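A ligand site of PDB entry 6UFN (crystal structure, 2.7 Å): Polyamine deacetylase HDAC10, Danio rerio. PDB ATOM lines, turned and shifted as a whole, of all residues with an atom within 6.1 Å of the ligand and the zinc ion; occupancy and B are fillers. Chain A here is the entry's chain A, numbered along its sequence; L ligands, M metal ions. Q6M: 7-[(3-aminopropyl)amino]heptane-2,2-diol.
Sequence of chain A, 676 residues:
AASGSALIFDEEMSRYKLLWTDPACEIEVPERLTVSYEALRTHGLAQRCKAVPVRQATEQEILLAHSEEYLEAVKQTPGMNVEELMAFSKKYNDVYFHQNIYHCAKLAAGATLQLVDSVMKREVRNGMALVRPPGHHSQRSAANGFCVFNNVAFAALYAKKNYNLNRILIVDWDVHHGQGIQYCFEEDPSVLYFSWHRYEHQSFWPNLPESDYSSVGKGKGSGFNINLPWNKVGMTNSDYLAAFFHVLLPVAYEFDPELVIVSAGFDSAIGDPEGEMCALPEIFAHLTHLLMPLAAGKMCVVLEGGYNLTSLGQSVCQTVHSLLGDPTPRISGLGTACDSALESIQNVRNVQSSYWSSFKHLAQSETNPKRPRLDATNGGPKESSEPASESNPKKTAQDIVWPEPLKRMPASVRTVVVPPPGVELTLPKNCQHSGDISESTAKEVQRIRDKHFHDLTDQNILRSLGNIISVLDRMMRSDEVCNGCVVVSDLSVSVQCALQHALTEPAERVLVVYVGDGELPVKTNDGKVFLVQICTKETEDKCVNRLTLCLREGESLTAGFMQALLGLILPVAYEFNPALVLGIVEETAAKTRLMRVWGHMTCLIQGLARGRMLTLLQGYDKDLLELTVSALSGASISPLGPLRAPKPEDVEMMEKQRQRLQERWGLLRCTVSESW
A ring nitrogen (NE2) of His 136 lies close to an oxygen (O03) of the ligand. OH of Tyr 307 sits close to O04 of the ligand. An oxygen (O03) of the ligand sits close to a ring nitrogen (NE2) of His 137, 2.8 Å away. A nitrogen (N10) of the ligand lies within salt-bridge range of the side-chain carboxylate (OD2) of Asp 94.
Of the 24 residues printed, 3 come within 4 Å of the zinc ion.
Merely in contact with the ligand: Glu 274 (3.3 Å), Gly 305 (3.3 Å), Ala 24 (3.4 Å), Gly 145 (3.4 Å), Trp 205 (3.5 Å), Pro 134 (3.5 Å), Phe 146 (3.6 Å), Pro 23 (3.7 Å) and Glu 304 (3.9 Å). Hydrophobic or aromatic side chains that line the ligand: Ala 24, Pro 134, His 136, His 137, Phe 146, His 176, Trp 205 and Tyr 307. 16 residues have an atom within 4 Å of the ligand: Pro 23, Ala 24, Asp 94, Pro 134, His 136, His 137, Gly 145, Phe 146, Asp 174, His 176, Trp 205, Asp 267, Glu 274, Glu 304, Gly 305 and Tyr 307. Along chain A the residues within 4 Å of the ligand span positions 23 to 307.
The zinc ion is bound by OD2 of Asp 267 (2.0 Å), O04 of the ligand (2.0 Å), OD2 of Asp 174 (2.1 Å), ND1 of His 176 (2.2 Å), O03 of the ligand (2.3 Å) and OD1 of Asp 174 (2.5 Å).
OD1 of Asp 267 sits at hydrogen-bond distance from N of Val 175 (3.0 Å). The side-chain carboxylate (OD1) of Asp 174 sits close to the backbone NH (N) of Gly 305, at 3.1 Å. NE2 of His 176 lies within hydrogen-bond range of OE2 of Glu 274, at 2.7 Å. NE2 of His 136 is in hydrogen-bond range of NE2 of His 137 (3.2 Å). The backbone NH (N) of His 136 lies within hydrogen-bond range of the side-chain sulfur (SG) of Cys 147. N of His 137 is in hydrogen-bond range of SG of Cys 147. The backbone carbonyl oxygen (O) of His 177 lies close to a ring nitrogen (ND1) of His 137 (3.1 Å). The backbone carbonyl oxygen of Pro 134 lies close to the side-chain sulfur of Cys 147.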
ATOM      1  N   PRO A  23      10.144 -13.122  -4.232  1.00  0.00           N
ATOM      2  CA  PRO A  23       8.915 -13.373  -3.462  1.00  0.00           C
ATOM      3  C   PRO A  23       7.635 -13.039  -4.221  1.00  0.00           C
ATOM      4  O   PRO A  23       6.572 -13.538  -3.845  1.00  0.00           O
ATOM      5  CB  PRO A  23       9.080 -12.471  -2.229  1.00  0.00           C
ATOM      6  CG  PRO A  23      10.558 -12.226  -2.131  1.00  0.00           C
ATOM      7  CD  PRO A  23      11.060 -12.198  -3.538  1.00  0.00           C
ATOM      8  N   ALA A  24       7.704 -12.219  -5.271  1.00  0.00           N
ATOM      9  CA  ALA A  24       6.503 -11.858  -6.014  1.00  0.00           C
ATOM     10  C   ALA A  24       6.074 -12.953  -6.973  1.00  0.00           C
ATOM     11  O   ALA A  24       4.882 -13.029  -7.319  1.00  0.00           O
ATOM     12  CB  ALA A  24       6.729 -10.551  -6.775  1.00  0.00           C
ATOM     13  N   CYS A  25       6.996 -13.804  -7.420  1.00  0.00           N
ATOM     14  CA  CYS A  25       6.706 -14.813  -8.436  1.00  0.00           C
ATOM     15  C   CYS A  25       6.823 -16.244  -7.920  1.00  0.00           C
ATOM     16  O   CYS A  25       6.594 -17.175  -8.702  1.00  0.00           O
ATOM     17  CB  CYS A  25       7.636 -14.624  -9.640  1.00  0.00           C
ATOM     18  SG  CYS A  25       7.392 -13.083 -10.552  1.00  0.00           S
ATOM     19  N   ILE A  27       4.935 -18.088  -6.349  1.00  0.00           N
ATOM     20  CA  ILE A  27       3.709 -18.875  -6.309  1.00  0.00           C
ATOM     21  C   ILE A  27       3.341 -19.474  -7.660  1.00  0.00           C
ATOM     22  O   ILE A  27       2.510 -20.385  -7.721  1.00  0.00           O
ATOM     23  CB  ILE A  27       2.538 -18.037  -5.787  1.00  0.00           C
ATOM     24  CG1 ILE A  27       2.350 -16.797  -6.662  1.00  0.00           C
ATOM     25  CG2 ILE A  27       2.766 -17.651  -4.330  1.00  0.00           C
ATOM     26  CD1 ILE A  27       1.159 -15.973  -6.288  1.00  0.00           C
ATOM     27  N   ASP A  94       6.470  -7.978 -12.221  1.00  0.00           N
ATOM     28  CA  ASP A  94       6.085  -9.247 -11.595  1.00  0.00           C
ATOM     29  C   ASP A  94       5.921 -10.370 -12.633  1.00  0.00           C
ATOM     30  O   ASP A  94       4.846 -10.950 -12.793  1.00  0.00           O
ATOM     31  CB  ASP A  94       4.812  -9.078 -10.758  1.00  0.00           C
ATOM     32  CG  ASP A  94       5.074  -8.381  -9.436  1.00  0.00           C
ATOM     33  OD1 ASP A  94       6.259  -8.094  -9.143  1.00  0.00           O
ATOM     34  OD2 ASP A  94       4.108  -8.136  -8.690  1.00  0.00           O
ATOM     35  N   PRO A 134      -0.182 -17.958 -17.796  1.00  0.00           N
ATOM     36  CA  PRO A 134      -1.456 -17.256 -18.018  1.00  0.00           C
ATOM     37  C   PRO A 134      -1.304 -16.119 -19.016  1.00  0.00           C
ATOM     38  O   PRO A 134      -0.213 -15.896 -19.550  1.00  0.00           O
ATOM     39  CB  PRO A 134      -1.821 -16.740 -16.615  1.00  0.00           C
ATOM     40  CG  PRO A 134      -0.519 -16.680 -15.888  1.00  0.00           C
ATOM     41  CD  PRO A 134       0.283 -17.837 -16.405  1.00  0.00           C
ATOM     42  N   GLY A 135      -2.376 -15.371 -19.266  1.00  0.00           N
ATOM     43  CA  GLY A 135      -2.318 -14.376 -20.314  1.00  0.00           C
ATOM     44  C   GLY A 135      -3.012 -13.052 -20.081  1.00  0.00           C
ATOM     45  O   GLY A 135      -2.641 -12.048 -20.705  1.00  0.00           O
ATOM     46  N   HIS A 136      -4.006 -13.008 -19.186  1.00  0.00           N
ATOM     47  CA  HIS A 136      -4.913 -11.856 -19.172  1.00  0.00           C
ATOM     48  C   HIS A 136      -4.242 -10.561 -18.690  1.00  0.00           C
ATOM     49  O   HIS A 136      -4.843  -9.498 -18.839  1.00  0.00           O
ATOM     50  CB  HIS A 136      -6.154 -12.164 -18.340  1.00  0.00           C
ATOM     51  CG  HIS A 136      -5.920 -12.227 -16.856  1.00  0.00           C
ATOM     52  ND1 HIS A 136      -6.944 -12.104 -15.941  1.00  0.00           N
ATOM     53  CD2 HIS A 136      -4.796 -12.426 -16.135  1.00  0.00           C
ATOM     54  CE1 HIS A 136      -6.450 -12.217 -14.721  1.00  0.00           C
ATOM     55  NE2 HIS A 136      -5.146 -12.405 -14.815  1.00  0.00           N
ATOM     56  N   HIS A 137      -3.027 -10.634 -18.154  1.00  0.00           N
ATOM     57  CA  HIS A 137      -2.283  -9.418 -17.830  1.00  0.00           C
ATOM     58  C   HIS A 137      -1.389  -8.936 -18.968  1.00  0.00           C
ATOM     59  O   HIS A 137      -0.984  -7.775 -18.976  1.00  0.00           O
ATOM     60  CB  HIS A 137      -1.424  -9.616 -16.578  1.00  0.00           C
ATOM     61  CG  HIS A 137      -2.212  -9.859 -15.330  1.00  0.00           C
ATOM     62  ND1 HIS A 137      -3.345  -9.137 -15.016  1.00  0.00           N
ATOM     63  CD2 HIS A 137      -2.028 -10.722 -14.308  1.00  0.00           C
ATOM     64  CE1 HIS A 137      -3.830  -9.559 -13.857  1.00  0.00           C
ATOM     65  NE2 HIS A 137      -3.043 -10.524 -13.404  1.00  0.00           N
ATOM     66  N   GLY A 145       2.595  -9.680 -14.893  1.00  0.00           N
ATOM     67  CA  GLY A 145       1.927 -10.591 -13.972  1.00  0.00           C
ATOM     68  C   GLY A 145       1.897 -12.039 -14.412  1.00  0.00           C
ATOM     69  O   GLY A 145       0.815 -12.592 -14.627  1.00  0.00           O
ATOM     70  N   PHE A 146       3.072 -12.652 -14.554  1.00  0.00           N
ATOM     71  CA  PHE A 146       3.270 -14.039 -14.965  1.00  0.00           C
ATOM     72  C   PHE A 146       2.840 -14.310 -16.409  1.00  0.00           C
ATOM     73  O   PHE A 146       2.975 -15.441 -16.866  1.00  0.00           O
ATOM     74  CB  PHE A 146       2.547 -15.048 -14.066  1.00  0.00           C
ATOM     75  CG  PHE A 146       2.720 -14.804 -12.590  1.00  0.00           C
ATOM     76  CD1 PHE A 146       3.909 -14.299 -12.087  1.00  0.00           C
ATOM     77  CD2 PHE A 146       1.688 -15.083 -11.709  1.00  0.00           C
ATOM     78  CE1 PHE A 146       4.059 -14.075 -10.724  1.00  0.00           C
ATOM     79  CE2 PHE A 146       1.826 -14.856 -10.352  1.00  0.00           C
ATOM     80  CZ  PHE A 146       3.014 -14.350  -9.863  1.00  0.00           C
ATOM     81  N   CYS A 147       2.322 -13.309 -17.114  1.00  0.00           N
ATOM     82  CA  CYS A 147       1.781 -13.502 -18.453  1.00  0.00           C
ATOM     83  C   CYS A 147       2.767 -13.016 -19.512  1.00  0.00           C
ATOM     84  O   CYS A 147       3.366 -11.943 -19.369  1.00  0.00           O
ATOM     85  CB  CYS A 147       0.450 -12.775 -18.613  1.00  0.00           C
ATOM     86  SG  CYS A 147      -0.770 -13.145 -17.324  1.00  0.00           S
ATOM     87  N   ASP A 174     -10.977 -14.574 -12.626  1.00  0.00           N
ATOM     88  CA  ASP A 174      -9.730 -14.536 -11.881  1.00  0.00           C
ATOM     89  C   ASP A 174      -9.765 -13.411 -10.864  1.00  0.00           C
ATOM     90  O   ASP A 174     -10.451 -12.403 -11.052  1.00  0.00           O
ATOM     91  CB  ASP A 174      -8.548 -14.358 -12.843  1.00  0.00           C
ATOM     92  CG  ASP A 174      -7.205 -14.378 -12.144  1.00  0.00           C
ATOM     93  OD1 ASP A 174      -6.545 -15.428 -12.141  1.00  0.00           O
ATOM     94  OD2 ASP A 174      -6.807 -13.328 -11.596  1.00  0.00           O
ATOM     95  N   VAL A 175      -9.035 -13.585  -9.763  1.00  0.00           N
ATOM     96  CA  VAL A 175      -9.094 -12.592  -8.687  1.00  0.00           C
ATOM     97  C   VAL A 175      -8.340 -11.316  -9.021  1.00  0.00           C
ATOM     98  O   VAL A 175      -8.522 -10.305  -8.345  1.00  0.00           O
ATOM     99  CB  VAL A 175      -8.563 -13.164  -7.357  1.00  0.00           C
ATOM    100  CG1 VAL A 175      -7.034 -13.208  -7.355  1.00  0.00           C
ATOM    101  CG2 VAL A 175      -9.097 -12.355  -6.182  1.00  0.00           C
ATOM    102  N   HIS A 176      -7.492 -11.339 -10.052  1.00  0.00           N
ATOM    103  CA  HIS A 176      -6.815 -10.141 -10.520  1.00  0.00           C
ATOM    104  C   HIS A 176      -7.535  -9.573 -11.743  1.00  0.00           C
ATOM    105  O   HIS A 176      -8.241 -10.287 -12.456  1.00  0.00           O
ATOM    106  CB  HIS A 176      -5.355 -10.442 -10.881  1.00  0.00           C
ATOM    107  CG  HIS A 176      -4.563 -11.030  -9.749  1.00  0.00           C
ATOM    108  ND1 HIS A 176      -4.546 -12.376  -9.463  1.00  0.00           N
ATOM    109  CD2 HIS A 176      -3.750 -10.433  -8.837  1.00  0.00           C
ATOM    110  CE1 HIS A 176      -3.764 -12.590  -8.426  1.00  0.00           C
ATOM    111  NE2 HIS A 176      -3.270 -11.440  -8.023  1.00  0.00           N
ATOM    112  N   HIS A 177      -7.351  -8.273 -11.968  1.00  0.00           N
ATOM    113  CA  HIS A 177      -7.977  -7.607 -13.101  1.00  0.00           C
ATOM    114  C   HIS A 177      -7.156  -7.865 -14.356  1.00  0.00           C
ATOM    115  O   HIS A 177      -5.966  -7.533 -14.415  1.00  0.00           O
ATOM    116  CB  HIS A 177      -8.094  -6.105 -12.846  1.00  0.00           C
ATOM    117  CG  HIS A 177      -8.655  -5.340 -14.008  1.00  0.00           C
ATOM    118  ND1 HIS A 177      -8.049  -4.213 -14.515  1.00  0.00           N
ATOM    119  CD2 HIS A 177      -9.758  -5.556 -14.765  1.00  0.00           C
ATOM    120  CE1 HIS A 177      -8.762  -3.755 -15.532  1.00  0.00           C
ATOM    121  NE2 HIS A 177      -9.799  -4.552 -15.705  1.00  0.00           N
ATOM    122  N   TRP A 205      -2.694  -5.062  -6.290  1.00  0.00           N
ATOM    123  CA  TRP A 205      -2.072  -5.180  -7.608  1.00  0.00           C
ATOM    124  C   TRP A 205      -3.129  -5.480  -8.671  1.00  0.00           C
ATOM    125  O   TRP A 205      -4.055  -6.271  -8.420  1.00  0.00           O
ATOM    126  CB  TRP A 205      -1.015  -6.287  -7.574  1.00  0.00           C
ATOM    127  CG  TRP A 205      -0.130  -6.337  -8.780  1.00  0.00           C
ATOM    128  CD1 TRP A 205       1.099  -5.761  -8.923  1.00  0.00           C
ATOM    129  CD2 TRP A 205      -0.399  -7.023 -10.015  1.00  0.00           C
ATOM    130  NE1 TRP A 205       1.609  -6.039 -10.161  1.00  0.00           N
ATOM    131  CE2 TRP A 205       0.701  -6.810 -10.855  1.00  0.00           C
ATOM    132  CE3 TRP A 205      -1.471  -7.791 -10.483  1.00  0.00           C
ATOM    133  CZ2 TRP A 205       0.773  -7.341 -12.144  1.00  0.00           C
ATOM    134  CZ3 TRP A 205      -1.404  -8.315 -11.757  1.00  0.00           C
ATOM    135  CH2 TRP A 205      -0.293  -8.081 -12.576  1.00  0.00           C
ATOM    136  N   GLY A 265      -9.452 -18.021 -13.761  1.00  0.00           N
ATOM    137  CA  GLY A 265      -8.481 -18.008 -12.691  1.00  0.00           C
ATOM    138  C   GLY A 265      -9.157 -18.412 -11.396  1.00  0.00           C
ATOM    139  O   GLY A 265     -10.193 -17.852 -11.019  1.00  0.00           O
ATOM    140  N   ASP A 267      -7.665 -18.376  -8.369  1.00  0.00           N
ATOM    141  CA  ASP A 267      -7.169 -17.672  -7.193  1.00  0.00           C
ATOM    142  C   ASP A 267      -8.252 -16.885  -6.496  1.00  0.00           C
ATOM    143  O   ASP A 267      -7.982 -16.283  -5.442  1.00  0.00           O
ATOM    144  CB  ASP A 267      -6.005 -16.752  -7.584  1.00  0.00           C
ATOM    145  CG  ASP A 267      -6.285 -15.970  -8.851  1.00  0.00           C
ATOM    146  OD1 ASP A 267      -7.419 -16.043  -9.364  1.00  0.00           O
ATOM    147  OD2 ASP A 267      -5.365 -15.278  -9.327  1.00  0.00           O
ATOM    148  N   GLU A 274      -3.257 -15.186  -2.886  1.00  0.00           N
ATOM    149  CA  GLU A 274      -3.384 -13.913  -3.587  1.00  0.00           C
ATOM    150  C   GLU A 274      -4.760 -13.282  -3.386  1.00  0.00           C
ATOM    151  O   GLU A 274      -4.864 -12.094  -3.077  1.00  0.00           O
ATOM    152  CB  GLU A 274      -3.116 -14.105  -5.080  1.00  0.00           C
ATOM    153  CG  GLU A 274      -1.660 -13.994  -5.476  1.00  0.00           C
ATOM    154  CD  GLU A 274      -1.094 -12.611  -5.280  1.00  0.00           C
ATOM    155  OE1 GLU A 274      -0.405 -12.384  -4.263  1.00  0.00           O
ATOM    156  OE2 GLU A 274      -1.349 -11.736  -6.132  1.00  0.00           O
ATOM    157  N   GLU A 304      -6.210 -19.449 -15.933  1.00  0.00           N
ATOM    158  CA  GLU A 304      -5.419 -18.267 -15.643  1.00  0.00           C
ATOM    159  C   GLU A 304      -4.644 -18.464 -14.349  1.00  0.00           C
ATOM    160  O   GLU A 304      -3.579 -19.084 -14.334  1.00  0.00           O
ATOM    161  CB  GLU A 304      -6.306 -17.028 -15.556  1.00  0.00           C
ATOM    162  CG  GLU A 304      -7.007 -16.659 -16.861  1.00  0.00           C
ATOM    163  CD  GLU A 304      -6.101 -15.883 -17.814  1.00  0.00           C
ATOM    164  OE1 GLU A 304      -4.967 -15.545 -17.422  1.00  0.00           O
ATOM    165  OE2 GLU A 304      -6.542 -15.601 -18.952  1.00  0.00           O
ATOM    166  N   GLY A 305      -5.177 -17.938 -13.245  1.00  0.00           N
ATOM    167  CA  GLY A 305      -4.535 -18.025 -11.949  1.00  0.00           C
ATOM    168  C   GLY A 305      -5.038 -19.194 -11.125  1.00  0.00           C
ATOM    169  O   GLY A 305      -5.761 -20.083 -11.597  1.00  0.00           O
ATOM    170  N   GLY A 306      -4.645 -19.188  -9.848  1.00  0.00           N
ATOM    171  CA  GLY A 306      -4.959 -20.270  -8.934  1.00  0.00           C
ATOM    172  C   GLY A 306      -3.703 -20.872  -8.336  1.00  0.00           C
ATOM    173  O   GLY A 306      -2.951 -21.559  -9.046  1.00  0.00           O
ATOM    174  N   TYR A 307      -3.462 -20.627  -7.050  1.00  0.00           N
ATOM    175  CA  TYR A 307      -2.164 -20.912  -6.467  1.00  0.00           C
ATOM    176  C   TYR A 307      -2.202 -21.770  -5.201  1.00  0.00           C
ATOM    177  O   TYR A 307      -1.152 -22.251  -4.780  1.00  0.00           O
ATOM    178  CB  TYR A 307      -1.421 -19.600  -6.174  1.00  0.00           C
ATOM    179  CG  TYR A 307      -1.376 -18.716  -7.390  1.00  0.00           C
ATOM    180  CD1 TYR A 307      -0.385 -18.889  -8.348  1.00  0.00           C
ATOM    181  CD2 TYR A 307      -2.340 -17.745  -7.608  1.00  0.00           C
ATOM    182  CE1 TYR A 307      -0.348 -18.101  -9.482  1.00  0.00           C
ATOM    183  CE2 TYR A 307      -2.316 -16.942  -8.741  1.00  0.00           C
ATOM    184  CZ  TYR A 307      -1.316 -17.124  -9.672  1.00  0.00           C
ATOM    185  OH  TYR A 307      -1.279 -16.336 -10.807  1.00  0.00           O
HETATM  186  C11 Q6M L   1       1.750 -10.235  -7.053  1.00  0.00           C
HETATM  187  C12 Q6M L   1       2.997 -10.505  -6.175  1.00  0.00           C
HETATM  188  C13 Q6M L   1       2.673 -11.479  -5.013  1.00  0.00           C
HETATM  189  C01 Q6M L   1      -3.195 -14.896 -13.925  1.00  0.00           C
HETATM  190  C02 Q6M L   1      -3.065 -14.113 -12.618  1.00  0.00           C
HETATM  191  C05 Q6M L   1      -1.655 -13.527 -12.412  1.00  0.00           C
HETATM  192  C06 Q6M L   1      -1.375 -12.956 -11.013  1.00  0.00           C
HETATM  193  C07 Q6M L   1      -0.320 -11.830 -11.015  1.00  0.00           C
HETATM  194  C08 Q6M L   1       0.368 -11.632  -9.659  1.00  0.00           C
HETATM  195  C09 Q6M L   1       0.915 -10.204  -9.416  1.00  0.00           C
HETATM  196  N10 Q6M L   1       2.090 -10.196  -8.504  1.00  0.00           N
HETATM  197  N14 Q6M L   1       3.654 -11.327  -3.923  1.00  0.00           N
HETATM  198  O03 Q6M L   1      -3.974 -13.044 -12.594  1.00  0.00           O
HETATM  199  O04 Q6M L   1      -3.346 -14.934 -11.530  1.00  0.00           O
HETATM  200 ZN    ZN M   1      -4.992 -14.027 -10.805  1.00  0.00          ZN
